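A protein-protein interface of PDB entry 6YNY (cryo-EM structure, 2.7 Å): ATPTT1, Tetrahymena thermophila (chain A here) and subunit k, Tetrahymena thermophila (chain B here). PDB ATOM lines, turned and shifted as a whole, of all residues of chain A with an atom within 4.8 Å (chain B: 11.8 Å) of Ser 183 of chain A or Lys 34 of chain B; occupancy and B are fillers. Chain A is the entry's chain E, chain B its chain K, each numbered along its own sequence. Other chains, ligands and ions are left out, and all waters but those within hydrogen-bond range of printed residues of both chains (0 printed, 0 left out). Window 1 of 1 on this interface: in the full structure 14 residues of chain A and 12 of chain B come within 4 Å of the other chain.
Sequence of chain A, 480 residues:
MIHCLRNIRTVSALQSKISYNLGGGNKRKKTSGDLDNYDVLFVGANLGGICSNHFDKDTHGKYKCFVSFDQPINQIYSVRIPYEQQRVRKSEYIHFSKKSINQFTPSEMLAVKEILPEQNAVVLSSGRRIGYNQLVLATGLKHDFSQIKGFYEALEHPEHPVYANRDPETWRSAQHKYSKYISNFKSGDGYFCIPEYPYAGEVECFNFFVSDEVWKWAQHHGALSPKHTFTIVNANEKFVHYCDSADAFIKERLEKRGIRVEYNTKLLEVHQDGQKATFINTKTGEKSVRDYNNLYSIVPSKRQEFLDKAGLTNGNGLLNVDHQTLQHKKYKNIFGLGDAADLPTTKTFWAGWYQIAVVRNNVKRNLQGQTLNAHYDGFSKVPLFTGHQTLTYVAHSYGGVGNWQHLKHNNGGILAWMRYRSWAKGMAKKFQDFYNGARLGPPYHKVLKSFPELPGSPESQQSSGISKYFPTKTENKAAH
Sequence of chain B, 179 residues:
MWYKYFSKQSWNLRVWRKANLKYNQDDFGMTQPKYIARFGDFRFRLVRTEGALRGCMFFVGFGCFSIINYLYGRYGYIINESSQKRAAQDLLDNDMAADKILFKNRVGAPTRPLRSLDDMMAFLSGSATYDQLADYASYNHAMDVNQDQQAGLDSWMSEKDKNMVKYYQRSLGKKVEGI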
ATOM      1  N   GLU A  84     -18.223   1.025 -26.538  1.00  0.00           N
ATOM      2  CA  GLU A  84     -19.554   1.404 -26.083  1.00  0.00           C
ATOM      3  C   GLU A  84     -20.492   0.208 -26.037  1.00  0.00           C
ATOM      4  O   GLU A  84     -21.456   0.207 -25.263  1.00  0.00           O
ATOM      5  CB  GLU A  84     -20.123   2.490 -26.990  1.00  0.00           C
ATOM      6  CG  GLU A  84     -19.326   3.775 -26.970  1.00  0.00           C
ATOM      7  CD  GLU A  84     -19.913   4.845 -27.866  1.00  0.00           C
ATOM      8  OE1 GLU A  84     -20.976   4.599 -28.471  1.00  0.00           O
ATOM      9  OE2 GLU A  84     -19.311   5.935 -27.964  1.00  0.00           O
ATOM     10  N   GLN A  85     -20.237  -0.808 -26.855  1.00  0.00           N
ATOM     11  CA  GLN A  85     -20.988  -2.053 -26.791  1.00  0.00           C
ATOM     12  C   GLN A  85     -20.460  -3.001 -25.727  1.00  0.00           C
ATOM     13  O   GLN A  85     -20.962  -4.123 -25.613  1.00  0.00           O
ATOM     14  CB  GLN A  85     -20.957  -2.755 -28.149  1.00  0.00           C
ATOM     15  CG  GLN A  85     -21.687  -2.026 -29.248  1.00  0.00           C
ATOM     16  CD  GLN A  85     -21.690  -2.805 -30.542  1.00  0.00           C
ATOM     17  OE1 GLN A  85     -20.870  -3.699 -30.741  1.00  0.00           O
ATOM     18  NE2 GLN A  85     -22.620  -2.479 -31.428  1.00  0.00           N
ATOM     19  N   GLN A  86     -19.464  -2.579 -24.952  1.00  0.00           N
ATOM     20  CA  GLN A  86     -18.871  -3.406 -23.907  1.00  0.00           C
ATOM     21  C   GLN A  86     -18.339  -4.720 -24.469  1.00  0.00           C
ATOM     22  O   GLN A  86     -18.344  -5.749 -23.789  1.00  0.00           O
ATOM     23  CB  GLN A  86     -19.865  -3.664 -22.774  1.00  0.00           C
ATOM     24  CG  GLN A  86     -20.091  -2.459 -21.886  1.00  0.00           C
ATOM     25  CD  GLN A  86     -20.752  -2.816 -20.581  1.00  0.00           C
ATOM     26  OE1 GLN A  86     -21.418  -3.842 -20.468  1.00  0.00           O
ATOM     27  NE2 GLN A  86     -20.562  -1.972 -19.578  1.00  0.00           N
ATOM     28  N   SER A 179     -21.485   3.476 -22.138  1.00  0.00           N
ATOM     29  CA  SER A 179     -22.269   2.387 -22.699  1.00  0.00           C
ATOM     30  C   SER A 179     -23.771   2.614 -22.604  1.00  0.00           C
ATOM     31  O   SER A 179     -24.536   1.764 -23.070  1.00  0.00           O
ATOM     32  CB  SER A 179     -21.905   1.082 -21.995  1.00  0.00           C
ATOM     33  OG  SER A 179     -22.136   1.176 -20.603  1.00  0.00           O
ATOM     34  N   LYS A 180     -24.212   3.723 -22.019  1.00  0.00           N
ATOM     35  CA  LYS A 180     -25.629   3.980 -21.813  1.00  0.00           C
ATOM     36  C   LYS A 180     -26.217   4.944 -22.833  1.00  0.00           C
ATOM     37  O   LYS A 180     -27.418   5.226 -22.772  1.00  0.00           O
ATOM     38  CB  LYS A 180     -25.865   4.523 -20.404  1.00  0.00           C
ATOM     39  CG  LYS A 180     -25.493   3.552 -19.304  1.00  0.00           C
ATOM     40  CD  LYS A 180     -26.003   4.013 -17.956  1.00  0.00           C
ATOM     41  CE  LYS A 180     -25.657   3.019 -16.863  1.00  0.00           C
ATOM     42  NZ  LYS A 180     -26.347   3.323 -15.585  1.00  0.00           N
ATOM     43  N   TYR A 181     -25.413   5.455 -23.763  1.00  0.00           N
ATOM     44  CA  TYR A 181     -25.944   6.385 -24.753  1.00  0.00           C
ATOM     45  C   TYR A 181     -27.015   5.724 -25.606  1.00  0.00           C
ATOM     46  O   TYR A 181     -28.063   6.321 -25.876  1.00  0.00           O
ATOM     47  CB  TYR A 181     -24.816   6.919 -25.632  1.00  0.00           C
ATOM     48  CG  TYR A 181     -25.304   7.601 -26.886  1.00  0.00           C
ATOM     49  CD1 TYR A 181     -26.027   8.780 -26.819  1.00  0.00           C
ATOM     50  CD2 TYR A 181     -25.042   7.068 -28.138  1.00  0.00           C
ATOM     51  CE1 TYR A 181     -26.479   9.404 -27.959  1.00  0.00           C
ATOM     52  CE2 TYR A 181     -25.488   7.688 -29.282  1.00  0.00           C
ATOM     53  CZ  TYR A 181     -26.205   8.856 -29.186  1.00  0.00           C
ATOM     54  OH  TYR A 181     -26.652   9.479 -30.325  1.00  0.00           O
ATOM     55  N   ILE A 182     -26.768   4.492 -26.044  1.00  0.00           N
ATOM     56  CA  ILE A 182     -27.716   3.808 -26.913  1.00  0.00           C
ATOM     57  C   ILE A 182     -28.821   3.151 -26.099  1.00  0.00           C
ATOM     58  O   ILE A 182     -29.992   3.171 -26.491  1.00  0.00           O
ATOM     59  CB  ILE A 182     -26.968   2.784 -27.783  1.00  0.00           C
ATOM     60  CG1 ILE A 182     -25.964   3.500 -28.688  1.00  0.00           C
ATOM     61  CG2 ILE A 182     -27.945   1.971 -28.594  1.00  0.00           C
ATOM     62  CD1 ILE A 182     -25.034   2.574 -29.426  1.00  0.00           C
ATOM     63  N   SER A 183     -28.471   2.560 -24.956  1.00  0.00           N
ATOM     64  CA  SER A 183     -29.459   1.842 -24.160  1.00  0.00           C
ATOM     65  C   SER A 183     -30.456   2.799 -23.524  1.00  0.00           C
ATOM     66  O   SER A 183     -31.673   2.619 -23.649  1.00  0.00           O
ATOM     67  CB  SER A 183     -28.753   1.014 -23.091  1.00  0.00           C
ATOM     68  OG  SER A 183     -27.791   0.160 -23.677  1.00  0.00           O
ATOM     69  N   ASN A 184     -29.961   3.820 -22.829  1.00  0.00           N
ATOM     70  CA  ASN A 184     -30.818   4.742 -22.087  1.00  0.00           C
ATOM     71  C   ASN A 184     -31.204   5.921 -22.981  1.00  0.00           C
ATOM     72  O   ASN A 184     -30.724   7.047 -22.842  1.00  0.00           O
ATOM     73  CB  ASN A 184     -30.126   5.202 -20.813  1.00  0.00           C
ATOM     74  CG  ASN A 184     -29.817   4.057 -19.877  1.00  0.00           C
ATOM     75  OD1 ASN A 184     -29.885   2.890 -20.261  1.00  0.00           O
ATOM     76  ND2 ASN A 184     -29.470   4.382 -18.641  1.00  0.00           N
ATOM     77  N   PHE A 185     -32.096   5.629 -23.919  1.00  0.00           N
ATOM     78  CA  PHE A 185     -32.713   6.616 -24.797  1.00  0.00           C
ATOM     79  C   PHE A 185     -34.213   6.386 -24.838  1.00  0.00           C
ATOM     80  O   PHE A 185     -34.841   6.313 -25.894  1.00  0.00           O
ATOM     81  CB  PHE A 185     -32.107   6.573 -26.194  1.00  0.00           C
ATOM     82  CG  PHE A 185     -32.724   7.555 -27.147  1.00  0.00           C
ATOM     83  CD1 PHE A 185     -33.001   8.845 -26.744  1.00  0.00           C
ATOM     84  CD2 PHE A 185     -33.026   7.186 -28.442  1.00  0.00           C
ATOM     85  CE1 PHE A 185     -33.569   9.745 -27.609  1.00  0.00           C
ATOM     86  CE2 PHE A 185     -33.596   8.088 -29.312  1.00  0.00           C
ATOM     87  CZ  PHE A 185     -33.866   9.367 -28.893  1.00  0.00           C
ATOM     88  N   LYS A 186     -34.803   6.239 -23.654  1.00  0.00           N
ATOM     89  CA  LYS A 186     -36.201   5.844 -23.558  1.00  0.00           C
ATOM     90  C   LYS A 186     -37.122   6.814 -24.283  1.00  0.00           C
ATOM     91  O   LYS A 186     -38.181   6.408 -24.775  1.00  0.00           O
ATOM     92  CB  LYS A 186     -36.599   5.738 -22.090  1.00  0.00           C
ATOM     93  CG  LYS A 186     -35.724   4.798 -21.281  1.00  0.00           C
ATOM     94  CD  LYS A 186     -35.803   3.382 -21.793  1.00  0.00           C
ATOM     95  CE  LYS A 186     -34.929   2.463 -20.981  1.00  0.00           C
ATOM     96  NZ  LYS A 186     -34.944   1.088 -21.523  1.00  0.00           N
ATOM     97  N   HIS A 388     -25.575  -3.383 -35.793  1.00  0.00           N
ATOM     98  CA  HIS A 388     -25.173  -3.773 -34.448  1.00  0.00           C
ATOM     99  C   HIS A 388     -23.974  -4.711 -34.478  1.00  0.00           C
ATOM    100  O   HIS A 388     -23.106  -4.649 -33.599  1.00  0.00           O
ATOM    101  CB  HIS A 388     -26.348  -4.429 -33.730  1.00  0.00           C
ATOM    102  CG  HIS A 388     -26.055  -4.814 -32.317  1.00  0.00           C
ATOM    103  ND1 HIS A 388     -25.665  -3.899 -31.363  1.00  0.00           N
ATOM    104  CD2 HIS A 388     -26.094  -6.014 -31.692  1.00  0.00           C
ATOM    105  CE1 HIS A 388     -25.475  -4.519 -30.214  1.00  0.00           C
ATOM    106  NE2 HIS A 388     -25.729  -5.803 -30.386  1.00  0.00           N
ATOM    107  N   TYR B  23     -31.061  -1.852  -8.529  1.00  0.00           N
ATOM    108  CA  TYR B  23     -30.048  -2.849  -8.843  1.00  0.00           C
ATOM    109  C   TYR B  23     -29.400  -2.495 -10.171  1.00  0.00           C
ATOM    110  O   TYR B  23     -30.090  -2.350 -11.185  1.00  0.00           O
ATOM    111  CB  TYR B  23     -30.644  -4.252  -8.892  1.00  0.00           C
ATOM    112  CG  TYR B  23     -29.645  -5.309  -9.293  1.00  0.00           C
ATOM    113  CD1 TYR B  23     -28.563  -5.606  -8.483  1.00  0.00           C
ATOM    114  CD2 TYR B  23     -29.782  -6.005 -10.480  1.00  0.00           C
ATOM    115  CE1 TYR B  23     -27.646  -6.563  -8.845  1.00  0.00           C
ATOM    116  CE2 TYR B  23     -28.869  -6.965 -10.849  1.00  0.00           C
ATOM    117  CZ  TYR B  23     -27.802  -7.239 -10.028  1.00  0.00           C
ATOM    118  OH  TYR B  23     -26.889  -8.198 -10.390  1.00  0.00           O
ATOM    119  N   ASN B  24     -28.075  -2.364 -10.161  1.00  0.00           N
ATOM    120  CA  ASN B  24     -27.318  -1.985 -11.349  1.00  0.00           C
ATOM    121  C   ASN B  24     -27.190  -3.197 -12.270  1.00  0.00           C
ATOM    122  O   ASN B  24     -26.143  -3.835 -12.390  1.00  0.00           O
ATOM    123  CB  ASN B  24     -25.963  -1.422 -10.956  1.00  0.00           C
ATOM    124  CG  ASN B  24     -25.244  -0.778 -12.111  1.00  0.00           C
ATOM    125  OD1 ASN B  24     -25.771  -0.692 -13.218  1.00  0.00           O
ATOM    126  ND2 ASN B  24     -24.038  -0.303 -11.855  1.00  0.00           N
ATOM    127  N   GLN B  25     -28.302  -3.510 -12.934  1.00  0.00           N
ATOM    128  CA  GLN B  25     -28.315  -4.589 -13.910  1.00  0.00           C
ATOM    129  C   GLN B  25     -27.519  -4.251 -15.160  1.00  0.00           C
ATOM    130  O   GLN B  25     -27.237  -5.152 -15.955  1.00  0.00           O
ATOM    131  CB  GLN B  25     -29.755  -4.930 -14.292  1.00  0.00           C
ATOM    132  CG  GLN B  25     -30.548  -3.770 -14.854  1.00  0.00           C
ATOM    133  CD  GLN B  25     -31.855  -4.193 -15.498  1.00  0.00           C
ATOM    134  OE1 GLN B  25     -32.401  -3.476 -16.332  1.00  0.00           O
ATOM    135  NE2 GLN B  25     -32.364  -5.354 -15.114  1.00  0.00           N
ATOM    136  N   ASP B  26     -27.151  -2.986 -15.349  1.00  0.00           N
ATOM    137  CA  ASP B  26     -26.364  -2.582 -16.503  1.00  0.00           C
ATOM    138  C   ASP B  26     -24.878  -2.857 -16.335  1.00  0.00           C
ATOM    139  O   ASP B  26     -24.145  -2.814 -17.329  1.00  0.00           O
ATOM    140  CB  ASP B  26     -26.572  -1.095 -16.776  1.00  0.00           C
ATOM    141  CG  ASP B  26     -27.970  -0.781 -17.266  1.00  0.00           C
ATOM    142  OD1 ASP B  26     -28.797  -1.714 -17.345  1.00  0.00           O
ATOM    143  OD2 ASP B  26     -28.242   0.397 -17.577  1.00  0.00           O
ATOM    144  N   ASP B  27     -24.416  -3.135 -15.116  1.00  0.00           N
ATOM    145  CA  ASP B  27     -23.009  -3.385 -14.858  1.00  0.00           C
ATOM    146  C   ASP B  27     -22.721  -4.777 -14.321  1.00  0.00           C
ATOM    147  O   ASP B  27     -21.555  -5.185 -14.318  1.00  0.00           O
ATOM    148  CB  ASP B  27     -22.457  -2.353 -13.867  1.00  0.00           C
ATOM    149  CG  ASP B  27     -22.425  -0.957 -14.443  1.00  0.00           C
ATOM    150  OD1 ASP B  27     -22.823  -0.788 -15.612  1.00  0.00           O
ATOM    151  OD2 ASP B  27     -22.000  -0.029 -13.725  1.00  0.00           O
ATOM    152  N   PHE B  28     -23.733  -5.512 -13.868  1.00  0.00           N
ATOM    153  CA  PHE B  28     -23.542  -6.854 -13.337  1.00  0.00           C
ATOM    154  C   PHE B  28     -24.610  -7.777 -13.893  1.00  0.00           C
ATOM    155  O   PHE B  28     -25.792  -7.426 -13.905  1.00  0.00           O
ATOM    156  CB  PHE B  28     -23.603  -6.869 -11.809  1.00  0.00           C
ATOM    157  CG  PHE B  28     -22.794  -5.796 -11.155  1.00  0.00           C
ATOM    158  CD1 PHE B  28     -23.411  -4.713 -10.566  1.00  0.00           C
ATOM    159  CD2 PHE B  28     -21.416  -5.870 -11.130  1.00  0.00           C
ATOM    160  CE1 PHE B  28     -22.674  -3.727  -9.964  1.00  0.00           C
ATOM    161  CE2 PHE B  28     -20.674  -4.882 -10.529  1.00  0.00           C
ATOM    162  CZ  PHE B  28     -21.305  -3.810  -9.945  1.00  0.00           C
ATOM    163  N   GLY B  29     -24.191  -8.948 -14.347  1.00  0.00           N
ATOM    164  CA  GLY B  29     -25.115  -9.988 -14.741  1.00  0.00           C
ATOM    165  C   GLY B  29     -25.255 -10.135 -16.240  1.00  0.00           C
ATOM    166  O   GLY B  29     -24.540  -9.533 -17.045  1.00  0.00           O
ATOM    167  N   MET B  30     -26.222 -10.976 -16.605  1.00  0.00           N
ATOM    168  CA  MET B  30     -26.509 -11.255 -18.004  1.00  0.00           C
ATOM    169  C   MET B  30     -26.950 -10.012 -18.759  1.00  0.00           C
ATOM    170  O   MET B  30     -26.903 -10.000 -19.994  1.00  0.00           O
ATOM    171  CB  MET B  30     -27.597 -12.324 -18.093  1.00  0.00           C
ATOM    172  CG  MET B  30     -27.279 -13.605 -17.345  1.00  0.00           C
ATOM    173  SD  MET B  30     -28.701 -14.696 -17.176  1.00  0.00           S
ATOM    174  CE  MET B  30     -29.050 -15.062 -18.889  1.00  0.00           C
ATOM    175  N   THR B  31     -27.383  -8.973 -18.051  1.00  0.00           N
ATOM    176  CA  THR B  31     -27.876  -7.752 -18.668  1.00  0.00           C
ATOM    177  C   THR B  31     -26.797  -6.702 -18.880  1.00  0.00           C
ATOM    178  O   THR B  31     -27.054  -5.704 -19.561  1.00  0.00           O
ATOM    179  CB  THR B  31     -28.988  -7.151 -17.807  1.00  0.00           C
ATOM    180  OG1 THR B  31     -28.503  -6.956 -16.475  1.00  0.00           O
ATOM    181  CG2 THR B  31     -30.181  -8.072 -17.765  1.00  0.00           C
ATOM    182  N   GLN B  32     -25.611  -6.892 -18.321  1.00  0.00           N
ATOM    183  CA  GLN B  32     -24.539  -5.918 -18.465  1.00  0.00           C
ATOM    184  C   GLN B  32     -24.056  -5.821 -19.908  1.00  0.00           C
ATOM    185  O   GLN B  32     -23.840  -4.709 -20.406  1.00  0.00           O
ATOM    186  CB  GLN B  32     -23.385  -6.273 -17.525  1.00  0.00           C
ATOM    187  CG  GLN B  32     -22.121  -5.470 -17.736  1.00  0.00           C
ATOM    188  CD  GLN B  32     -21.159  -6.122 -18.703  1.00  0.00           C
ATOM    189  OE1 GLN B  32     -21.467  -7.142 -19.316  1.00  0.00           O
ATOM    190  NE2 GLN B  32     -19.978  -5.538 -18.837  1.00  0.00           N
ATOM    191  N   PRO B  33     -23.869  -6.934 -20.614  1.00  0.00           N
ATOM    192  CA  PRO B  33     -23.422  -6.843 -22.011  1.00  0.00           C
ATOM    193  C   PRO B  33     -24.407  -6.055 -22.857  1.00  0.00           C
ATOM    194  O   PRO B  33     -25.593  -6.379 -22.928  1.00  0.00           O
ATOM    195  CB  PRO B  33     -23.337  -8.308 -22.447  1.00  0.00           C
ATOM    196  CG  PRO B  33     -23.138  -9.055 -21.192  1.00  0.00           C
ATOM    197  CD  PRO B  33     -23.949  -8.335 -20.171  1.00  0.00           C
ATOM    198  N   LYS B  34     -23.903  -5.011 -23.505  1.00  0.00           N
ATOM    199  CA  LYS B  34     -24.717  -4.169 -24.367  1.00  0.00           C
ATOM    200  C   LYS B  34     -24.650  -4.588 -25.826  1.00  0.00           C
ATOM    201  O   LYS B  34     -25.346  -3.998 -26.657  1.00  0.00           O
ATOM    202  CB  LYS B  34     -24.283  -2.710 -24.230  1.00  0.00           C
ATOM    203  CG  LYS B  34     -24.228  -2.218 -22.797  1.00  0.00           C
ATOM    204  CD  LYS B  34     -25.596  -2.218 -22.147  1.00  0.00           C
ATOM    205  CE  LYS B  34     -25.507  -1.904 -20.668  1.00  0.00           C
ATOM    206  NZ  LYS B  34     -24.973  -0.549 -20.421  1.00  0.00           N
ATOM    207  N   TYR B  35     -23.836  -5.589 -26.157  1.00  0.00           N
ATOM    208  CA  TYR B  35     -23.733  -6.098 -27.513  1.00  0.00           C
ATOM    209  C   TYR B  35     -24.767  -7.170 -27.811  1.00  0.00           C
ATOM    210  O   TYR B  35     -24.568  -7.977 -28.726  1.00  0.00           O
ATOM    211  CB  TYR B  35     -22.326  -6.642 -27.764  1.00  0.00           C
ATOM    212  CG  TYR B  35     -21.893  -7.739 -26.822  1.00  0.00           C
ATOM    213  CD1 TYR B  35     -22.358  -9.034 -26.972  1.00  0.00           C
ATOM    214  CD2 TYR B  35     -21.004  -7.482 -25.793  1.00  0.00           C
ATOM    215  CE1 TYR B  35     -21.960 -10.036 -26.117  1.00  0.00           C
ATOM    216  CE2 TYR B  35     -20.598  -8.478 -24.937  1.00  0.00           C
ATOM    217  CZ  TYR B  35     -21.079  -9.753 -25.103  1.00  0.00           C
ATOM    218  OH  TYR B  35     -20.678 -10.752 -24.250  1.00  0.00           O
ATOM    219  N   ILE B  36     -25.858  -7.196 -27.069  1.00  0.00           N
ATOM    220  CA  ILE B  36     -26.875  -8.221 -27.245  1.00  0.00           C
ATOM    221  C   ILE B  36     -27.770  -7.847 -28.417  1.00  0.00           C
ATOM    222  O   ILE B  36     -27.986  -6.668 -28.718  1.00  0.00           O
ATOM    223  CB  ILE B  36     -27.674  -8.403 -25.940  1.00  0.00           C
ATOM    224  CG1 ILE B  36     -28.306  -9.787 -25.897  1.00  0.00           C
ATOM    225  CG2 ILE B  36     -28.735  -7.337 -25.812  1.00  0.00           C
ATOM    226  CD1 ILE B  36     -28.893 -10.123 -24.567  1.00  0.00           C
ATOM    227  N   ALA B  37     -28.298  -8.864 -29.087  1.00  0.00           N
ATOM    228  CA  ALA B  37     -29.002  -8.690 -30.346  1.00  0.00           C
ATOM    229  C   ALA B  37     -30.501  -8.513 -30.110  1.00  0.00           C
ATOM    230  O   ALA B  37     -30.960  -8.275 -28.990  1.00  0.00           O
ATOM    231  CB  ALA B  37     -28.714  -9.871 -31.266  1.00  0.00           C
ATOM    232  N   ARG B  38     -31.280  -8.632 -31.187  1.00  0.00           N
ATOM    233  CA  ARG B  38     -32.712  -8.373 -31.114  1.00  0.00           C
ATOM    234  C   ARG B  38     -33.413  -9.376 -30.210  1.00  0.00           C
ATOM    235  O   ARG B  38     -34.310  -9.010 -29.442  1.00  0.00           O
ATOM    236  CB  ARG B  38     -33.303  -8.414 -32.523  1.00  0.00           C
ATOM    237  CG  ARG B  38     -34.661  -7.759 -32.674  1.00  0.00           C
ATOM    238  CD  ARG B  38     -35.034  -7.628 -34.138  1.00  0.00           C
ATOM    239  NE  ARG B  38     -36.151  -6.714 -34.357  1.00  0.00           N
ATOM    240  CZ  ARG B  38     -37.431  -7.067 -34.364  1.00  0.00           C
ATOM    241  NH1 ARG B  38     -37.789  -8.325 -34.163  1.00  0.00           N
ATOM    242  NH2 ARG B  38     -38.359  -6.148 -34.577  1.00  0.00           N
ATOM    243  N   PHE B  39     -33.018 -10.645 -30.286  1.00  0.00           N
ATOM    244  CA  PHE B  39     -33.690 -11.677 -29.505  1.00  0.00           C
ATOM    245  C   PHE B  39     -33.372 -11.538 -28.022  1.00  0.00           C
ATOM    246  O   PHE B  39     -34.272 -11.582 -27.176  1.00  0.00           O
ATOM    247  CB  PHE B  39     -33.290 -13.056 -30.018  1.00  0.00           C
ATOM    248  CG  PHE B  39     -33.867 -14.187 -29.223  1.00  0.00           C
ATOM    249  CD1 PHE B  39     -35.190 -14.548 -29.374  1.00  0.00           C
ATOM    250  CD2 PHE B  39     -33.082 -14.895 -28.334  1.00  0.00           C
ATOM    251  CE1 PHE B  39     -35.722 -15.588 -28.646  1.00  0.00           C
ATOM    252  CE2 PHE B  39     -33.608 -15.934 -27.606  1.00  0.00           C
ATOM    253  CZ  PHE B  39     -34.929 -16.282 -27.762  1.00  0.00           C
ATOM    254  N   GLY B  40     -32.094 -11.366 -27.688  1.00  0.00           N
ATOM    255  CA  GLY B  40     -31.719 -11.234 -26.292  1.00  0.00           C
ATOM    256  C   GLY B  40     -32.273  -9.985 -25.644  1.00  0.00           C
ATOM    257  O   GLY B  40     -32.564  -9.983 -24.445  1.00  0.00           O
ATOM    258  N   ASP B  41     -32.427  -8.911 -26.416  1.00  0.00           N
ATOM    259  CA  ASP B  41     -33.011  -7.692 -25.871  1.00  0.00           C
ATOM    260  C   ASP B  41     -34.505  -7.859 -25.643  1.00  0.00           C
ATOM    261  O   ASP B  41     -35.030  -7.450 -24.602  1.00  0.00           O
ATOM    262  CB  ASP B  41     -32.733  -6.518 -26.808  1.00  0.00           C
ATOM    263  CG  ASP B  41     -33.117  -5.180 -26.207  1.00  0.00           C
ATOM    264  OD1 ASP B  41     -34.167  -5.097 -25.539  1.00  0.00           O
ATOM    265  OD2 ASP B  41     -32.364  -4.205 -26.404  1.00  0.00           O
ATOM    266  N   PHE B  42     -35.207  -8.461 -26.602  1.00  0.00           N
ATOM    267  CA  PHE B  42     -36.634  -8.691 -26.436  1.00  0.00           C
ATOM    268  C   PHE B  42     -36.920  -9.684 -25.323  1.00  0.00           C
ATOM    269  O   PHE B  42     -38.012  -9.658 -24.748  1.00  0.00           O
ATOM    270  CB  PHE B  42     -37.238  -9.191 -27.747  1.00  0.00           C
ATOM    271  CG  PHE B  42     -38.724  -9.344 -27.708  1.00  0.00           C
ATOM    272  CD1 PHE B  42     -39.547  -8.244 -27.840  1.00  0.00           C
ATOM    273  CD2 PHE B  42     -39.300 -10.588 -27.546  1.00  0.00           C
ATOM    274  CE1 PHE B  42     -40.913  -8.381 -27.806  1.00  0.00           C
ATOM    275  CE2 PHE B  42     -40.668 -10.729 -27.511  1.00  0.00           C
ATOM    276  CZ  PHE B  42     -41.476  -9.624 -27.642  1.00  0.00           C
ATOM    277  N   PHE B  44     -35.056 -10.053 -22.324  1.00  0.00           N
ATOM    278  CA  PHE B  44     -34.976  -9.308 -21.073  1.00  0.00           C
ATOM    279  C   PHE B  44     -36.059  -8.243 -20.984  1.00  0.00           C
ATOM    280  O   PHE B  44     -36.532  -7.929 -19.886  1.00  0.00           O
ATOM    281  CB  PHE B  44     -33.602  -8.659 -20.931  1.00  0.00           C
ATOM    282  CG  PHE B  44     -32.492  -9.627 -20.656  1.00  0.00           C
ATOM    283  CD1 PHE B  44     -32.635 -10.622 -19.707  1.00  0.00           C
ATOM    284  CD2 PHE B  44     -31.299  -9.537 -21.344  1.00  0.00           C
ATOM    285  CE1 PHE B  44     -31.612 -11.505 -19.455  1.00  0.00           C
ATOM    286  CE2 PHE B  44     -30.274 -10.417 -21.094  1.00  0.00           C
ATOM    287  CZ  PHE B  44     -30.429 -11.402 -20.150  1.00  0.00           C
ATOM    288  N   ARG B  45     -36.459  -7.675 -22.121  1.00  0.00           N
ATOM    289  CA  ARG B  45     -37.527  -6.685 -22.118  1.00  0.00           C
ATOM    290  C   ARG B  45     -38.813  -7.255 -21.537  1.00  0.00           C
ATOM    291  O   ARG B  45     -39.583  -6.528 -20.900  1.00  0.00           O
ATOM    292  CB  ARG B  45     -37.759  -6.182 -23.540  1.00  0.00           C
ATOM    293  CG  ARG B  45     -38.894  -5.201 -23.702  1.00  0.00           C
ATOM    294  CD  ARG B  45     -38.585  -3.854 -23.098  1.00  0.00           C
ATOM    295  NE  ARG B  45     -39.653  -2.903 -23.386  1.00  0.00           N
ATOM    296  CZ  ARG B  45     -40.711  -2.699 -22.612  1.00  0.00           C
ATOM    297  NH1 ARG B  45     -41.624  -1.815 -22.973  1.00  0.00           N
ATOM    298  NH2 ARG B  45     -40.862  -3.363 -21.479  1.00  0.00           N
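The backbone carbonyl oxygen of Gln 85 of chain A is in hydrogen-bond range of the backbone NH of Tyr 35 of chain B, 3.3 Å away.
The backbone carbonyl oxygen (O) of Gln 32 of chain B lies close to the side-chain amide oxygen (OE1) of Gln 86 of chain A (2.6 Å).
OG of Ser 179 of chain A sits at hydrogen-bond distance from NZ of Lys 34 of chain B.
A ring nitrogen (NE2) of His 388 of chain A is in hydrogen-bond range of the backbone carbonyl oxygen (O) of Tyr 35 of chain B, at 3.0 Å.
A ring nitrogen (NE2) of His 388 of chain A is in hydrogen-bond range of the backbone carbonyl oxygen of Ile 36 of chain B.
NE2 of Gln 85 of chain A lies within hydrogen-bond range of O of His 388 of chain A (3.1 Å).
The side-chain amide oxygen (OD1) of Asn 24 of chain B lies close to the backbone NH (N) of Asp 26 of chain B (3.4 Å).
The backbone carbonyl oxygen of Gln 25 of chain B sits at hydrogen-bond distance from the backbone NH of Gln 32 of chain B (3.4 Å).
Gln 85 of chain A touches Lys 34 of chain B (O to C, 3.7 Å).
Gln 86 of chain A touches Pro 33 of chain B.
Lys 34 of chain B touches Gln 86 of chain A (CG to OE1, 3.99 Å).
Tyr 35 of chain B touches Gln 86 of chain A (CE2 to O, 3.7 Å).
Ser 183 of chain A touches Lys 34 of chain B.
CE1 of His 388 of chain A touches O of Lys 34 of chain B (3.6 Å).
Ser 183 of chain A touches just one residue of chain B: Lys 34 (3.6 Å).
Of chain B, only Lys 34 and Tyr 35 come within 4 Å of Gln 85 of chain A.
Ser 179 of chain A touches one residue of chain B.
Of chain B, only Asp 26 comes within 4 Å of Lys 180 of chain A.
No residue of chain B comes within 4 Å of Ile 182 of chain A.
No residue of chain B comes within 4 Å of Lys 186 of chain A.
Of the printed residues of chain A, Ile 36 of chain B touches His 388 (2.9 Å).
Printed residues of chain A within 4 Å of Tyr 35 of chain B: Gln 85, Gln 86 and His 388.
Of the printed residues of chain A, Gln 32 of chain B touches Gln 86 (2.6 Å).
Printed residues of chain A within 4 Å of Pro 33 of chain B: Gln 86.
The nearest residue of chain B that does not touch Ser 183 of chain A is Asp 26 of chain B (5.6 Å).
The nearest printed residue of chain A that does not touch Lys 34 of chain B is Glu 84 of chain A (4.2 Å).
Of the 22 printed residues of chain B, 6 touch a printed residue of chain A.
Printed residues of chain B that touch a printed residue of chain A: Asp 26, Gln 32, Pro 33, Lys 34, Tyr 35 and Ile 36.
Among the printed residues, no Asp or Glu carboxylate lies within 4 Å of a Lys or Arg side-chain nitrogen of the other chain.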
